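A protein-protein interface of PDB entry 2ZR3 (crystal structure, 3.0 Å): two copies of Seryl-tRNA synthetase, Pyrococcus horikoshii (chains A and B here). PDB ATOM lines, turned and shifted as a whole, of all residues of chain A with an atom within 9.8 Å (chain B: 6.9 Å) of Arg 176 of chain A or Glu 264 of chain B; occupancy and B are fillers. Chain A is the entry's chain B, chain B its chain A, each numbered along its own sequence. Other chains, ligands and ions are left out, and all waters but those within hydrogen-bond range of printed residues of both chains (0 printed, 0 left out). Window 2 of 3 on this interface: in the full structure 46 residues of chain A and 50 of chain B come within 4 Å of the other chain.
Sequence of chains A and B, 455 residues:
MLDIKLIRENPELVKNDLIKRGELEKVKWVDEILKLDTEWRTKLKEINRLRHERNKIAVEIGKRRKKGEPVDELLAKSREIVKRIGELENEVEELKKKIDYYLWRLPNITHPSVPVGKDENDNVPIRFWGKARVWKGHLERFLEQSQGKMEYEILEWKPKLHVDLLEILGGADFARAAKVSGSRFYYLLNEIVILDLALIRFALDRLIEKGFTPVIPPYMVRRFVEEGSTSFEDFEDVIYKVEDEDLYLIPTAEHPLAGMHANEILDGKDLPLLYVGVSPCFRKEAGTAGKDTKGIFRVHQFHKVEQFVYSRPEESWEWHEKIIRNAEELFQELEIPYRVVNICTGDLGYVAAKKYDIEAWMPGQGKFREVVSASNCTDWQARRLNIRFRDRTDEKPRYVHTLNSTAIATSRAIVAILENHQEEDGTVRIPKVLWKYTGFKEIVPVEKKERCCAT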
ATOM      1  N   GLU A 167     -20.662  -0.746 -28.874  1.00  0.00           N
ATOM      2  CA  GLU A 167     -21.974  -0.124 -28.976  1.00  0.00           C
ATOM      3  C   GLU A 167     -23.126  -1.090 -29.235  1.00  0.00           C
ATOM      4  O   GLU A 167     -24.183  -0.966 -28.607  1.00  0.00           O
ATOM      5  CB  GLU A 167     -21.946   0.967 -30.043  1.00  0.00           C
ATOM      6  CG  GLU A 167     -22.089   2.382 -29.479  1.00  0.00           C
ATOM      7  CD  GLU A 167     -23.537   2.744 -29.137  1.00  0.00           C
ATOM      8  OE1 GLU A 167     -24.324   3.008 -30.080  1.00  0.00           O
ATOM      9  OE2 GLU A 167     -23.891   2.762 -27.932  1.00  0.00           O
ATOM     10  N   ALA A 172     -20.509   0.203 -23.284  1.00  0.00           N
ATOM     11  CA  ALA A 172     -19.825   1.474 -23.083  1.00  0.00           C
ATOM     12  C   ALA A 172     -20.646   2.641 -23.614  1.00  0.00           C
ATOM     13  O   ALA A 172     -21.429   2.473 -24.537  1.00  0.00           O
ATOM     14  CB  ALA A 172     -18.467   1.441 -23.787  1.00  0.00           C
ATOM     15  N   ASP A 173     -20.461   3.820 -23.020  1.00  0.00           N
ATOM     16  CA  ASP A 173     -21.144   5.049 -23.440  1.00  0.00           C
ATOM     17  C   ASP A 173     -20.021   6.088 -23.490  1.00  0.00           C
ATOM     18  O   ASP A 173     -19.458   6.450 -22.458  1.00  0.00           O
ATOM     19  CB  ASP A 173     -22.211   5.459 -22.411  1.00  0.00           C
ATOM     20  CG  ASP A 173     -22.937   6.781 -22.767  1.00  0.00           C
ATOM     21  OD1 ASP A 173     -22.273   7.788 -23.135  1.00  0.00           O
ATOM     22  OD2 ASP A 173     -24.186   6.822 -22.645  1.00  0.00           O
ATOM     23  N   PHE A 174     -19.679   6.542 -24.696  1.00  0.00           N
ATOM     24  CA  PHE A 174     -18.608   7.519 -24.865  1.00  0.00           C
ATOM     25  C   PHE A 174     -19.116   8.945 -24.920  1.00  0.00           C
ATOM     26  O   PHE A 174     -18.453   9.875 -24.462  1.00  0.00           O
ATOM     27  CB  PHE A 174     -17.810   7.239 -26.142  1.00  0.00           C
ATOM     28  CG  PHE A 174     -17.091   5.919 -26.139  1.00  0.00           C
ATOM     29  CD1 PHE A 174     -17.705   4.769 -26.635  1.00  0.00           C
ATOM     30  CD2 PHE A 174     -15.789   5.824 -25.647  1.00  0.00           C
ATOM     31  CE1 PHE A 174     -17.032   3.550 -26.644  1.00  0.00           C
ATOM     32  CE2 PHE A 174     -15.111   4.606 -25.653  1.00  0.00           C
ATOM     33  CZ  PHE A 174     -15.735   3.468 -26.153  1.00  0.00           C
ATOM     34  N   ALA A 175     -20.292   9.118 -25.501  1.00  0.00           N
ATOM     35  CA  ALA A 175     -20.860  10.442 -25.623  1.00  0.00           C
ATOM     36  C   ALA A 175     -20.939  11.107 -24.262  1.00  0.00           C
ATOM     37  O   ALA A 175     -20.428  12.216 -24.060  1.00  0.00           O
ATOM     38  CB  ALA A 175     -22.237  10.352 -26.240  1.00  0.00           C
ATOM     39  N   ARG A 176     -21.563  10.413 -23.318  1.00  0.00           N
ATOM     40  CA  ARG A 176     -21.726  10.969 -21.991  1.00  0.00           C
ATOM     41  C   ARG A 176     -20.427  11.192 -21.227  1.00  0.00           C
ATOM     42  O   ARG A 176     -20.328  12.114 -20.423  1.00  0.00           O
ATOM     43  CB  ARG A 176     -22.685  10.101 -21.197  1.00  0.00           C
ATOM     44  CG  ARG A 176     -24.097  10.121 -21.758  1.00  0.00           C
ATOM     45  CD  ARG A 176     -25.028   9.304 -20.869  1.00  0.00           C
ATOM     46  NE  ARG A 176     -26.435   9.630 -21.070  1.00  0.00           N
ATOM     47  CZ  ARG A 176     -27.196   9.117 -22.027  1.00  0.00           C
ATOM     48  NH1 ARG A 176     -28.465   9.487 -22.128  1.00  0.00           N
ATOM     49  NH2 ARG A 176     -26.695   8.222 -22.868  1.00  0.00           N
ATOM     50  N   ALA A 177     -19.424  10.364 -21.481  1.00  0.00           N
ATOM     51  CA  ALA A 177     -18.154  10.539 -20.801  1.00  0.00           C
ATOM     52  C   ALA A 177     -17.507  11.830 -21.298  1.00  0.00           C
ATOM     53  O   ALA A 177     -16.918  12.589 -20.522  1.00  0.00           O
ATOM     54  CB  ALA A 177     -17.239   9.342 -21.059  1.00  0.00           C
ATOM     55  N   ALA A 178     -17.623  12.088 -22.596  1.00  0.00           N
ATOM     56  CA  ALA A 178     -17.047  13.299 -23.169  1.00  0.00           C
ATOM     57  C   ALA A 178     -17.723  14.512 -22.543  1.00  0.00           C
ATOM     58  O   ALA A 178     -17.102  15.561 -22.355  1.00  0.00           O
ATOM     59  CB  ALA A 178     -17.234  13.314 -24.659  1.00  0.00           C
ATOM     60  N   LYS A 179     -18.997  14.361 -22.210  1.00  0.00           N
ATOM     61  CA  LYS A 179     -19.727  15.451 -21.586  1.00  0.00           C
ATOM     62  C   LYS A 179     -19.180  15.718 -20.197  1.00  0.00           C
ATOM     63  O   LYS A 179     -18.918  16.848 -19.808  1.00  0.00           O
ATOM     64  CB  LYS A 179     -21.215  15.098 -21.465  1.00  0.00           C
ATOM     65  CG  LYS A 179     -21.997  16.062 -20.587  1.00  0.00           C
ATOM     66  CD  LYS A 179     -23.494  15.771 -20.599  1.00  0.00           C
ATOM     67  CE  LYS A 179     -23.819  14.383 -20.086  1.00  0.00           C
ATOM     68  NZ  LYS A 179     -25.286  14.151 -20.123  1.00  0.00           N
ATOM     69  N   VAL A 180     -19.012  14.629 -19.466  1.00  0.00           N
ATOM     70  CA  VAL A 180     -18.562  14.620 -18.090  1.00  0.00           C
ATOM     71  C   VAL A 180     -17.074  14.821 -17.837  1.00  0.00           C
ATOM     72  O   VAL A 180     -16.694  15.410 -16.823  1.00  0.00           O
ATOM     73  CB  VAL A 180     -19.011  13.300 -17.455  1.00  0.00           C
ATOM     74  CG1 VAL A 180     -18.043  12.858 -16.411  1.00  0.00           C
ATOM     75  CG2 VAL A 180     -20.395  13.464 -16.879  1.00  0.00           C
ATOM     76  N   SER A 181     -16.226  14.340 -18.742  1.00  0.00           N
ATOM     77  CA  SER A 181     -14.790  14.463 -18.524  1.00  0.00           C
ATOM     78  C   SER A 181     -14.017  14.951 -19.737  1.00  0.00           C
ATOM     79  O   SER A 181     -12.975  15.575 -19.609  1.00  0.00           O
ATOM     80  CB  SER A 181     -14.211  13.111 -18.077  1.00  0.00           C
ATOM     81  OG  SER A 181     -14.926  12.559 -16.980  1.00  0.00           O
ATOM     82  N   GLY A 182     -14.518  14.664 -20.922  1.00  0.00           N
ATOM     83  CA  GLY A 182     -13.798  15.079 -22.102  1.00  0.00           C
ATOM     84  C   GLY A 182     -13.490  13.873 -22.957  1.00  0.00           C
ATOM     85  O   GLY A 182     -13.928  12.757 -22.658  1.00  0.00           O
ATOM     86  N   SER A 183     -12.749  14.086 -24.037  1.00  0.00           N
ATOM     87  CA  SER A 183     -12.415  12.981 -24.916  1.00  0.00           C
ATOM     88  C   SER A 183     -11.456  12.028 -24.209  1.00  0.00           C
ATOM     89  O   SER A 183     -10.901  12.348 -23.151  1.00  0.00           O
ATOM     90  CB  SER A 183     -11.783  13.498 -26.215  1.00  0.00           C
ATOM     91  OG  SER A 183     -10.485  14.025 -26.000  1.00  0.00           O
ATOM     92  N   PHE A 185     -12.025   9.437 -22.511  1.00  0.00           N
ATOM     93  CA  PHE A 185     -12.569   8.962 -21.239  1.00  0.00           C
ATOM     94  C   PHE A 185     -13.758   8.120 -21.680  1.00  0.00           C
ATOM     95  O   PHE A 185     -14.176   8.203 -22.832  1.00  0.00           O
ATOM     96  CB  PHE A 185     -13.025  10.104 -20.318  1.00  0.00           C
ATOM     97  CG  PHE A 185     -11.954  10.588 -19.377  1.00  0.00           C
ATOM     98  CD1 PHE A 185     -11.291  11.792 -19.606  1.00  0.00           C
ATOM     99  CD2 PHE A 185     -11.562   9.806 -18.290  1.00  0.00           C
ATOM    100  CE1 PHE A 185     -10.245  12.212 -18.766  1.00  0.00           C
ATOM    101  CE2 PHE A 185     -10.519  10.217 -17.450  1.00  0.00           C
ATOM    102  CZ  PHE A 185      -9.859  11.424 -17.690  1.00  0.00           C
ATOM    103  N   TYR A 186     -14.309   7.310 -20.793  1.00  0.00           N
ATOM    104  CA  TYR A 186     -15.417   6.464 -21.190  1.00  0.00           C
ATOM    105  C   TYR A 186     -16.147   5.927 -19.987  1.00  0.00           C
ATOM    106  O   TYR A 186     -15.721   6.096 -18.847  1.00  0.00           O
ATOM    107  CB  TYR A 186     -14.882   5.268 -21.947  1.00  0.00           C
ATOM    108  CG  TYR A 186     -13.832   4.559 -21.135  1.00  0.00           C
ATOM    109  CD1 TYR A 186     -12.507   4.970 -21.182  1.00  0.00           C
ATOM    110  CD2 TYR A 186     -14.177   3.538 -20.234  1.00  0.00           C
ATOM    111  CE1 TYR A 186     -11.546   4.399 -20.352  1.00  0.00           C
ATOM    112  CE2 TYR A 186     -13.219   2.957 -19.393  1.00  0.00           C
ATOM    113  CZ  TYR A 186     -11.905   3.404 -19.459  1.00  0.00           C
ATOM    114  OH  TYR A 186     -10.947   2.916 -18.605  1.00  0.00           O
ATOM    115  N   TYR A 187     -17.251   5.256 -20.265  1.00  0.00           N
ATOM    116  CA  TYR A 187     -18.021   4.621 -19.232  1.00  0.00           C
ATOM    117  C   TYR A 187     -18.104   3.201 -19.727  1.00  0.00           C
ATOM    118  O   TYR A 187     -18.434   2.988 -20.881  1.00  0.00           O
ATOM    119  CB  TYR A 187     -19.452   5.152 -19.155  1.00  0.00           C
ATOM    120  CG  TYR A 187     -19.668   6.468 -18.450  1.00  0.00           C
ATOM    121  CD1 TYR A 187     -19.742   7.653 -19.175  1.00  0.00           C
ATOM    122  CD2 TYR A 187     -19.895   6.523 -17.072  1.00  0.00           C
ATOM    123  CE1 TYR A 187     -20.045   8.859 -18.562  1.00  0.00           C
ATOM    124  CE2 TYR A 187     -20.198   7.732 -16.438  1.00  0.00           C
ATOM    125  CZ  TYR A 187     -20.273   8.899 -17.198  1.00  0.00           C
ATOM    126  OH  TYR A 187     -20.576  10.117 -16.625  1.00  0.00           O
ATOM    127  N   LEU A 188     -17.798   2.238 -18.874  1.00  0.00           N
ATOM    128  CA  LEU A 188     -17.913   0.829 -19.235  1.00  0.00           C
ATOM    129  C   LEU A 188     -19.222   0.332 -18.612  1.00  0.00           C
ATOM    130  O   LEU A 188     -19.581   0.725 -17.492  1.00  0.00           O
ATOM    131  CB  LEU A 188     -16.721   0.033 -18.689  1.00  0.00           C
ATOM    132  CG  LEU A 188     -15.617  -0.388 -19.673  1.00  0.00           C
ATOM    133  CD1 LEU A 188     -15.494   0.628 -20.816  1.00  0.00           C
ATOM    134  CD2 LEU A 188     -14.290  -0.556 -18.909  1.00  0.00           C
ATOM    135  N   LEU A 189     -19.937  -0.523 -19.338  1.00  0.00           N
ATOM    136  CA  LEU A 189     -21.215  -1.046 -18.850  1.00  0.00           C
ATOM    137  C   LEU A 189     -21.392  -2.551 -18.980  1.00  0.00           C
ATOM    138  O   LEU A 189     -20.696  -3.242 -19.742  1.00  0.00           O
ATOM    139  CB  LEU A 189     -22.373  -0.375 -19.586  1.00  0.00           C
ATOM    140  CG  LEU A 189     -22.242   1.138 -19.706  1.00  0.00           C
ATOM    141  CD1 LEU A 189     -23.202   1.669 -20.735  1.00  0.00           C
ATOM    142  CD2 LEU A 189     -22.482   1.763 -18.350  1.00  0.00           C
ATOM    143  N   LYS A 294     -11.926   8.169 -29.996  1.00  0.00           N
ATOM    144  CA  LYS A 294     -13.132   7.389 -29.702  1.00  0.00           C
ATOM    145  C   LYS A 294     -12.826   5.887 -29.614  1.00  0.00           C
ATOM    146  O   LYS A 294     -12.433   5.247 -30.594  1.00  0.00           O
ATOM    147  CB  LYS A 294     -14.210   7.626 -30.754  1.00  0.00           C
ATOM    148  CG  LYS A 294     -15.426   6.742 -30.549  1.00  0.00           C
ATOM    149  CD  LYS A 294     -16.288   7.228 -29.409  1.00  0.00           C
ATOM    150  CE  LYS A 294     -17.361   8.167 -29.930  1.00  0.00           C
ATOM    151  NZ  LYS A 294     -16.791   9.340 -30.654  1.00  0.00           N
ATOM    152  N   PRO B 218     -15.526   7.418 -15.458  1.00  0.00           N
ATOM    153  CA  PRO B 218     -14.217   8.066 -15.475  1.00  0.00           C
ATOM    154  C   PRO B 218     -13.847   8.462 -14.041  1.00  0.00           C
ATOM    155  O   PRO B 218     -14.698   8.877 -13.259  1.00  0.00           O
ATOM    156  CB  PRO B 218     -14.427   9.266 -16.412  1.00  0.00           C
ATOM    157  CG  PRO B 218     -15.907   9.468 -16.442  1.00  0.00           C
ATOM    158  CD  PRO B 218     -16.449   8.072 -16.397  1.00  0.00           C
ATOM    159  N   GLY B 259     -23.475  13.050 -12.934  1.00  0.00           N
ATOM    160  CA  GLY B 259     -23.224  13.872 -14.099  1.00  0.00           C
ATOM    161  C   GLY B 259     -23.455  13.117 -15.405  1.00  0.00           C
ATOM    162  O   GLY B 259     -23.387  13.692 -16.497  1.00  0.00           O
ATOM    163  N   MET B 260     -23.733  11.826 -15.304  1.00  0.00           N
ATOM    164  CA  MET B 260     -23.971  11.024 -16.493  1.00  0.00           C
ATOM    165  C   MET B 260     -25.147  11.514 -17.362  1.00  0.00           C
ATOM    166  O   MET B 260     -25.102  11.429 -18.587  1.00  0.00           O
ATOM    167  CB  MET B 260     -24.193   9.567 -16.085  1.00  0.00           C
ATOM    168  CG  MET B 260     -24.581   8.648 -17.214  1.00  0.00           C
ATOM    169  SD  MET B 260     -24.592   6.928 -16.682  1.00  0.00           S
ATOM    170  CE  MET B 260     -23.069   6.428 -17.315  1.00  0.00           C
ATOM    171  N   HIS B 261     -26.199  12.028 -16.735  1.00  0.00           N
ATOM    172  CA  HIS B 261     -27.365  12.504 -17.479  1.00  0.00           C
ATOM    173  C   HIS B 261     -27.574  14.004 -17.267  1.00  0.00           C
ATOM    174  O   HIS B 261     -28.698  14.490 -17.164  1.00  0.00           O
ATOM    175  CB  HIS B 261     -28.615  11.705 -17.059  1.00  0.00           C
ATOM    176  CG  HIS B 261     -28.562  10.255 -17.449  1.00  0.00           C
ATOM    177  ND1 HIS B 261     -28.657   9.830 -18.759  1.00  0.00           N
ATOM    178  CD2 HIS B 261     -28.404   9.134 -16.703  1.00  0.00           C
ATOM    179  CE1 HIS B 261     -28.562   8.512 -18.802  1.00  0.00           C
ATOM    180  NE2 HIS B 261     -28.407   8.064 -17.569  1.00  0.00           N
ATOM    181  N   ALA B 262     -26.472  14.739 -17.195  1.00  0.00           N
ATOM    182  CA  ALA B 262     -26.548  16.179 -17.008  1.00  0.00           C
ATOM    183  C   ALA B 262     -27.144  16.786 -18.272  1.00  0.00           C
ATOM    184  O   ALA B 262     -26.793  16.384 -19.378  1.00  0.00           O
ATOM    185  CB  ALA B 262     -25.164  16.744 -16.759  1.00  0.00           C
ATOM    186  N   ASN B 263     -28.048  17.746 -18.096  1.00  0.00           N
ATOM    187  CA  ASN B 263     -28.714  18.433 -19.202  1.00  0.00           C
ATOM    188  C   ASN B 263     -29.586  17.540 -20.064  1.00  0.00           C
ATOM    189  O   ASN B 263     -29.656  17.742 -21.263  1.00  0.00           O
ATOM    190  CB  ASN B 263     -27.702  19.129 -20.117  1.00  0.00           C
ATOM    191  CG  ASN B 263     -26.986  20.270 -19.441  1.00  0.00           C
ATOM    192  OD1 ASN B 263     -27.615  21.179 -18.893  1.00  0.00           O
ATOM    193  ND2 ASN B 263     -25.656  20.242 -19.482  1.00  0.00           N
ATOM    194  N   GLU B 264     -30.252  16.553 -19.479  1.00  0.00           N
ATOM    195  CA  GLU B 264     -31.113  15.686 -20.275  1.00  0.00           C
ATOM    196  C   GLU B 264     -32.552  15.741 -19.805  1.00  0.00           C
ATOM    197  O   GLU B 264     -32.881  16.399 -18.816  1.00  0.00           O
ATOM    198  CB  GLU B 264     -30.663  14.227 -20.204  1.00  0.00           C
ATOM    199  CG  GLU B 264     -29.299  13.909 -20.788  1.00  0.00           C
ATOM    200  CD  GLU B 264     -29.028  12.413 -20.775  1.00  0.00           C
ATOM    201  OE1 GLU B 264     -27.906  12.005 -21.123  1.00  0.00           O
ATOM    202  OE2 GLU B 264     -29.950  11.644 -20.415  1.00  0.00           O
ATOM    203  N   ILE B 265     -33.408  15.047 -20.547  1.00  0.00           N
ATOM    204  CA  ILE B 265     -34.818  14.943 -20.210  1.00  0.00           C
ATOM    205  C   ILE B 265     -35.160  13.485 -20.399  1.00  0.00           C
ATOM    206  O   ILE B 265     -35.296  13.004 -21.515  1.00  0.00           O
ATOM    207  CB  ILE B 265     -35.708  15.795 -21.114  1.00  0.00           C
ATOM    208  CG1 ILE B 265     -35.372  17.281 -20.915  1.00  0.00           C
ATOM    209  CG2 ILE B 265     -37.167  15.523 -20.772  1.00  0.00           C
ATOM    210  CD1 ILE B 265     -36.079  18.222 -21.857  1.00  0.00           C
ATOM    211  N   LEU B 266     -35.277  12.780 -19.287  1.00  0.00           N
ATOM    212  CA  LEU B 266     -35.556  11.363 -19.322  1.00  0.00           C
ATOM    213  C   LEU B 266     -36.988  11.029 -19.694  1.00  0.00           C
ATOM    214  O   LEU B 266     -37.894  11.857 -19.544  1.00  0.00           O
ATOM    215  CB  LEU B 266     -35.217  10.745 -17.961  1.00  0.00           C
ATOM    216  CG  LEU B 266     -33.754  10.854 -17.525  1.00  0.00           C
ATOM    217  CD1 LEU B 266     -33.603  10.304 -16.117  1.00  0.00           C
ATOM    218  CD2 LEU B 266     -32.857  10.102 -18.513  1.00  0.00           C
ATOM    219  N   LEU B 273     -33.987   4.570 -12.996  1.00  0.00           N
ATOM    220  CA  LEU B 273     -32.735   4.170 -13.625  1.00  0.00           C
ATOM    221  C   LEU B 273     -31.905   3.641 -12.454  1.00  0.00           C
ATOM    222  O   LEU B 273     -31.765   4.321 -11.428  1.00  0.00           O
ATOM    223  CB  LEU B 273     -32.037   5.366 -14.277  1.00  0.00           C
ATOM    224  CG  LEU B 273     -32.802   6.087 -15.388  1.00  0.00           C
ATOM    225  CD1 LEU B 273     -31.990   7.263 -15.922  1.00  0.00           C
ATOM    226  CD2 LEU B 273     -33.095   5.103 -16.501  1.00  0.00           C
ATOM    227  N   TYR B 275     -28.234   2.306 -11.297  1.00  0.00           N
ATOM    228  CA  TYR B 275     -26.820   2.084 -11.534  1.00  0.00           C
ATOM    229  C   TYR B 275     -26.013   1.628 -10.297  1.00  0.00           C
ATOM    230  O   TYR B 275     -26.266   2.060  -9.176  1.00  0.00           O
ATOM    231  CB  TYR B 275     -26.215   3.367 -12.095  1.00  0.00           C
ATOM    232  CG  TYR B 275     -26.787   3.833 -13.421  1.00  0.00           C
ATOM    233  CD1 TYR B 275     -26.630   3.081 -14.577  1.00  0.00           C
ATOM    234  CD2 TYR B 275     -27.398   5.079 -13.536  1.00  0.00           C
ATOM    235  CE1 TYR B 275     -27.054   3.566 -15.826  1.00  0.00           C
ATOM    236  CE2 TYR B 275     -27.824   5.572 -14.773  1.00  0.00           C
ATOM    237  CZ  TYR B 275     -27.643   4.812 -15.909  1.00  0.00           C
ATOM    238  OH  TYR B 275     -28.016   5.314 -17.128  1.00  0.00           O
ATOM    239  N   LEU B 385     -27.758  20.004 -12.007  1.00  0.00           N
ATOM    240  CA  LEU B 385     -27.291  19.389 -13.237  1.00  0.00           C
ATOM    241  C   LEU B 385     -28.317  19.436 -14.355  1.00  0.00           C
ATOM    242  O   LEU B 385     -28.041  18.977 -15.465  1.00  0.00           O
ATOM    243  CB  LEU B 385     -26.902  17.940 -12.963  1.00  0.00           C
ATOM    244  CG  LEU B 385     -25.753  17.794 -11.972  1.00  0.00           C
ATOM    245  CD1 LEU B 385     -25.527  16.324 -11.624  1.00  0.00           C
ATOM    246  CD2 LEU B 385     -24.510  18.413 -12.590  1.00  0.00           C
ATOM    247  N   ASN B 386     -29.498  19.980 -14.055  1.00  0.00           N
ATOM    248  CA  ASN B 386     -30.578  20.099 -15.035  1.00  0.00           C
ATOM    249  C   ASN B 386     -31.021  18.721 -15.557  1.00  0.00           C
ATOM    250  O   ASN B 386     -31.075  18.474 -16.763  1.00  0.00           O
ATOM    251  CB  ASN B 386     -30.121  21.033 -16.180  1.00  0.00           C
ATOM    252  CG  ASN B 386     -31.175  21.226 -17.268  1.00  0.00           C
ATOM    253  OD1 ASN B 386     -32.385  21.205 -17.010  1.00  0.00           O
ATOM    254  ND2 ASN B 386     -30.708  21.445 -18.494  1.00  0.00           N
ATOM    255  N   ILE B 387     -31.349  17.836 -14.622  1.00  0.00           N
ATOM    256  CA  ILE B 387     -31.796  16.491 -14.948  1.00  0.00           C
ATOM    257  C   ILE B 387     -33.306  16.439 -14.742  1.00  0.00           C
ATOM    258  O   ILE B 387     -33.776  16.278 -13.619  1.00  0.00           O
ATOM    259  CB  ILE B 387     -31.128  15.457 -14.025  1.00  0.00           C
ATOM    260  CG1 ILE B 387     -29.615  15.569 -14.136  1.00  0.00           C
ATOM    261  CG2 ILE B 387     -31.557  14.054 -14.397  1.00  0.00           C
ATOM    262  CD1 ILE B 387     -28.900  14.519 -13.339  1.00  0.00           C
ATOM    263  N   ARG B 388     -34.057  16.576 -15.830  1.00  0.00           N
ATOM    264  CA  ARG B 388     -35.520  16.567 -15.781  1.00  0.00           C
ATOM    265  C   ARG B 388     -36.086  15.338 -16.484  1.00  0.00           C
ATOM    266  O   ARG B 388     -35.331  14.538 -17.035  1.00  0.00           O
ATOM    267  CB  ARG B 388     -36.061  17.832 -16.448  1.00  0.00           C
ATOM    268  CG  ARG B 388     -35.532  19.112 -15.840  1.00  0.00           C
ATOM    269  CD  ARG B 388     -35.949  20.325 -16.648  1.00  0.00           C
ATOM    270  NE  ARG B 388     -35.224  20.418 -17.910  1.00  0.00           N
ATOM    271  CZ  ARG B 388     -35.553  21.246 -18.893  1.00  0.00           C
ATOM    272  NH1 ARG B 388     -34.838  21.270 -20.010  1.00  0.00           N
ATOM    273  NH2 ARG B 388     -36.606  22.042 -18.766  1.00  0.00           N
ATOM    274  N   PHE B 389     -37.409  15.185 -16.461  1.00  0.00           N
ATOM    275  CA  PHE B 389     -38.057  14.048 -17.123  1.00  0.00           C
ATOM    276  C   PHE B 389     -39.508  14.380 -17.466  1.00  0.00           C
ATOM    277  O   PHE B 389     -40.085  15.305 -16.893  1.00  0.00           O
ATOM    278  CB  PHE B 389     -38.008  12.801 -16.230  1.00  0.00           C
ATOM    279  CG  PHE B 389     -39.034  12.797 -15.142  1.00  0.00           C
ATOM    280  CD1 PHE B 389     -39.058  13.810 -14.190  1.00  0.00           C
ATOM    281  CD2 PHE B 389     -40.000  11.804 -15.089  1.00  0.00           C
ATOM    282  CE1 PHE B 389     -40.034  13.836 -13.201  1.00  0.00           C
ATOM    283  CE2 PHE B 389     -40.978  11.816 -14.109  1.00  0.00           C
ATOM    284  CZ  PHE B 389     -40.998  12.835 -13.161  1.00  0.00           C
ATOM    285  N   PRO B 397     -41.372  19.629 -18.473  1.00  0.00           N
ATOM    286  CA  PRO B 397     -40.524  18.585 -17.907  1.00  0.00           C
ATOM    287  C   PRO B 397     -40.256  18.924 -16.434  1.00  0.00           C
ATOM    288  O   PRO B 397     -39.973  20.077 -16.099  1.00  0.00           O
ATOM    289  CB  PRO B 397     -39.271  18.647 -18.785  1.00  0.00           C
ATOM    290  CG  PRO B 397     -39.228  20.078 -19.228  1.00  0.00           C
ATOM    291  CD  PRO B 397     -40.669  20.368 -19.539  1.00  0.00           C
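The side-chain carboxylate (OE1) of Glu 264 of chain B is in salt-bridge range of the guanidinium group (NH1) of Arg 176 of chain A, at 2.8 Å. ND1 of His 261 of chain B lies within hydrogen-bond range of NE of Arg 176 of chain A (3.2 Å). The backbone carbonyl oxygen (O) of Ala 262 of chain B sits at hydrogen-bond distance from the side-chain amino group (NZ) of Lys 179 of chain A, at 2.8 Å. The backbone carbonyl oxygen (O) of Met 260 of chain B lies close to the guanidinium group (NE) of Arg 176 of chain A (3.3 Å). The side-chain amino group (NZ) of Lys 179 of chain A is in hydrogen-bond range of the backbone carbonyl oxygen (O) of Met 260 of chain B (3.1 Å). The side-chain carboxylate (OE1) of Glu 264 of chain B lies within salt-bridge range of the side-chain amino group (NZ) of Lys 179 of chain A, at 3.5 Å.
The backbone NH of Glu 264 of chain B is in hydrogen-bond range of the backbone carbonyl oxygen of Asn 386 of chain B (3.4 Å). The backbone carbonyl oxygen (O) of Glu 264 of chain B lies within hydrogen-bond range of the backbone NH (N) of Arg 388 of chain B (3.2 Å). The backbone carbonyl oxygen of Tyr 187 of chain A is in hydrogen-bond range of the backbone NH of Asp 173 of chain A (3.1 Å). A ring nitrogen (NE2) of His 261 of chain B sits at hydrogen-bond distance from the side-chain hydroxyl (OH) of Tyr 275 of chain B, 2.8 Å away. The side-chain carboxylate of Glu 264 of chain B is in hydrogen-bond range of a ring nitrogen (ND1) of His 261 of chain B (2.8 Å). NH2 of Arg 176 of chain A lies within salt-bridge range of OD2 of Asp 173 of chain A.
O of Gly 259 of chain B touches CE of Lys 179 of chain A, at 3.7 Å. His 261 of chain B touches Lys 179 of chain A (C to NZ, 3.7 Å). O of Gly 259 of chain B touches CG2 of Val 180 of chain A (3.0 Å). Pro 218 of chain B touches Ser 181 of chain A (CG to OG, 3.3 Å). Pro 218 of chain B touches Phe 185 of chain A. O of Tyr 186 of chain A touches CD of Pro 218 of chain B, at 3.2 Å. Pro 218 of chain B touches Tyr 187 of chain A (CD to CE2, 3.8 Å). Met 260 of chain B touches Tyr 187 of chain A.
Arg 176 of chain A touches three residues of chain B. Ala 178 of chain A touches none of the printed residues of chain B. Of the printed residues of chain B, Tyr 187 of chain A touches Pro 218 (3.8 Å) and Met 260 (3.2 Å). Leu 189 of chain A touches none of the printed residues of chain B. Of the printed residues of chain A, Pro 218 of chain B touches Ser 181, Phe 185, Tyr 186 and Tyr 187. Of chain A, only Arg 176 (3.2 Å) and Lys 179 (3.7 Å) come within 4 Å of His 261 of chain B. Of chain A, only Arg 176 and Lys 179 come within 4 Å of Glu 264 of chain B.
Of the 17 printed residues of chain B, 6 touch a printed residue of chain A. Printed residues of chain B that touch a printed residue of chain A: Pro 218, Gly 259, Met 260, His 261, Ala 262 and Glu 264. Among the printed residues, Asp or Glu carboxylates within 4 Å of a Lys or Arg side-chain nitrogen of the other chain: Arg 176 of chain A with Glu 264 of chain B and Lys 179 of chain A with Glu 264 of chain B.
No position is printed for both chains. Of the 14 pairs that touch across the chains among the printed residues, none has its exchanged pair printed and touching as well.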
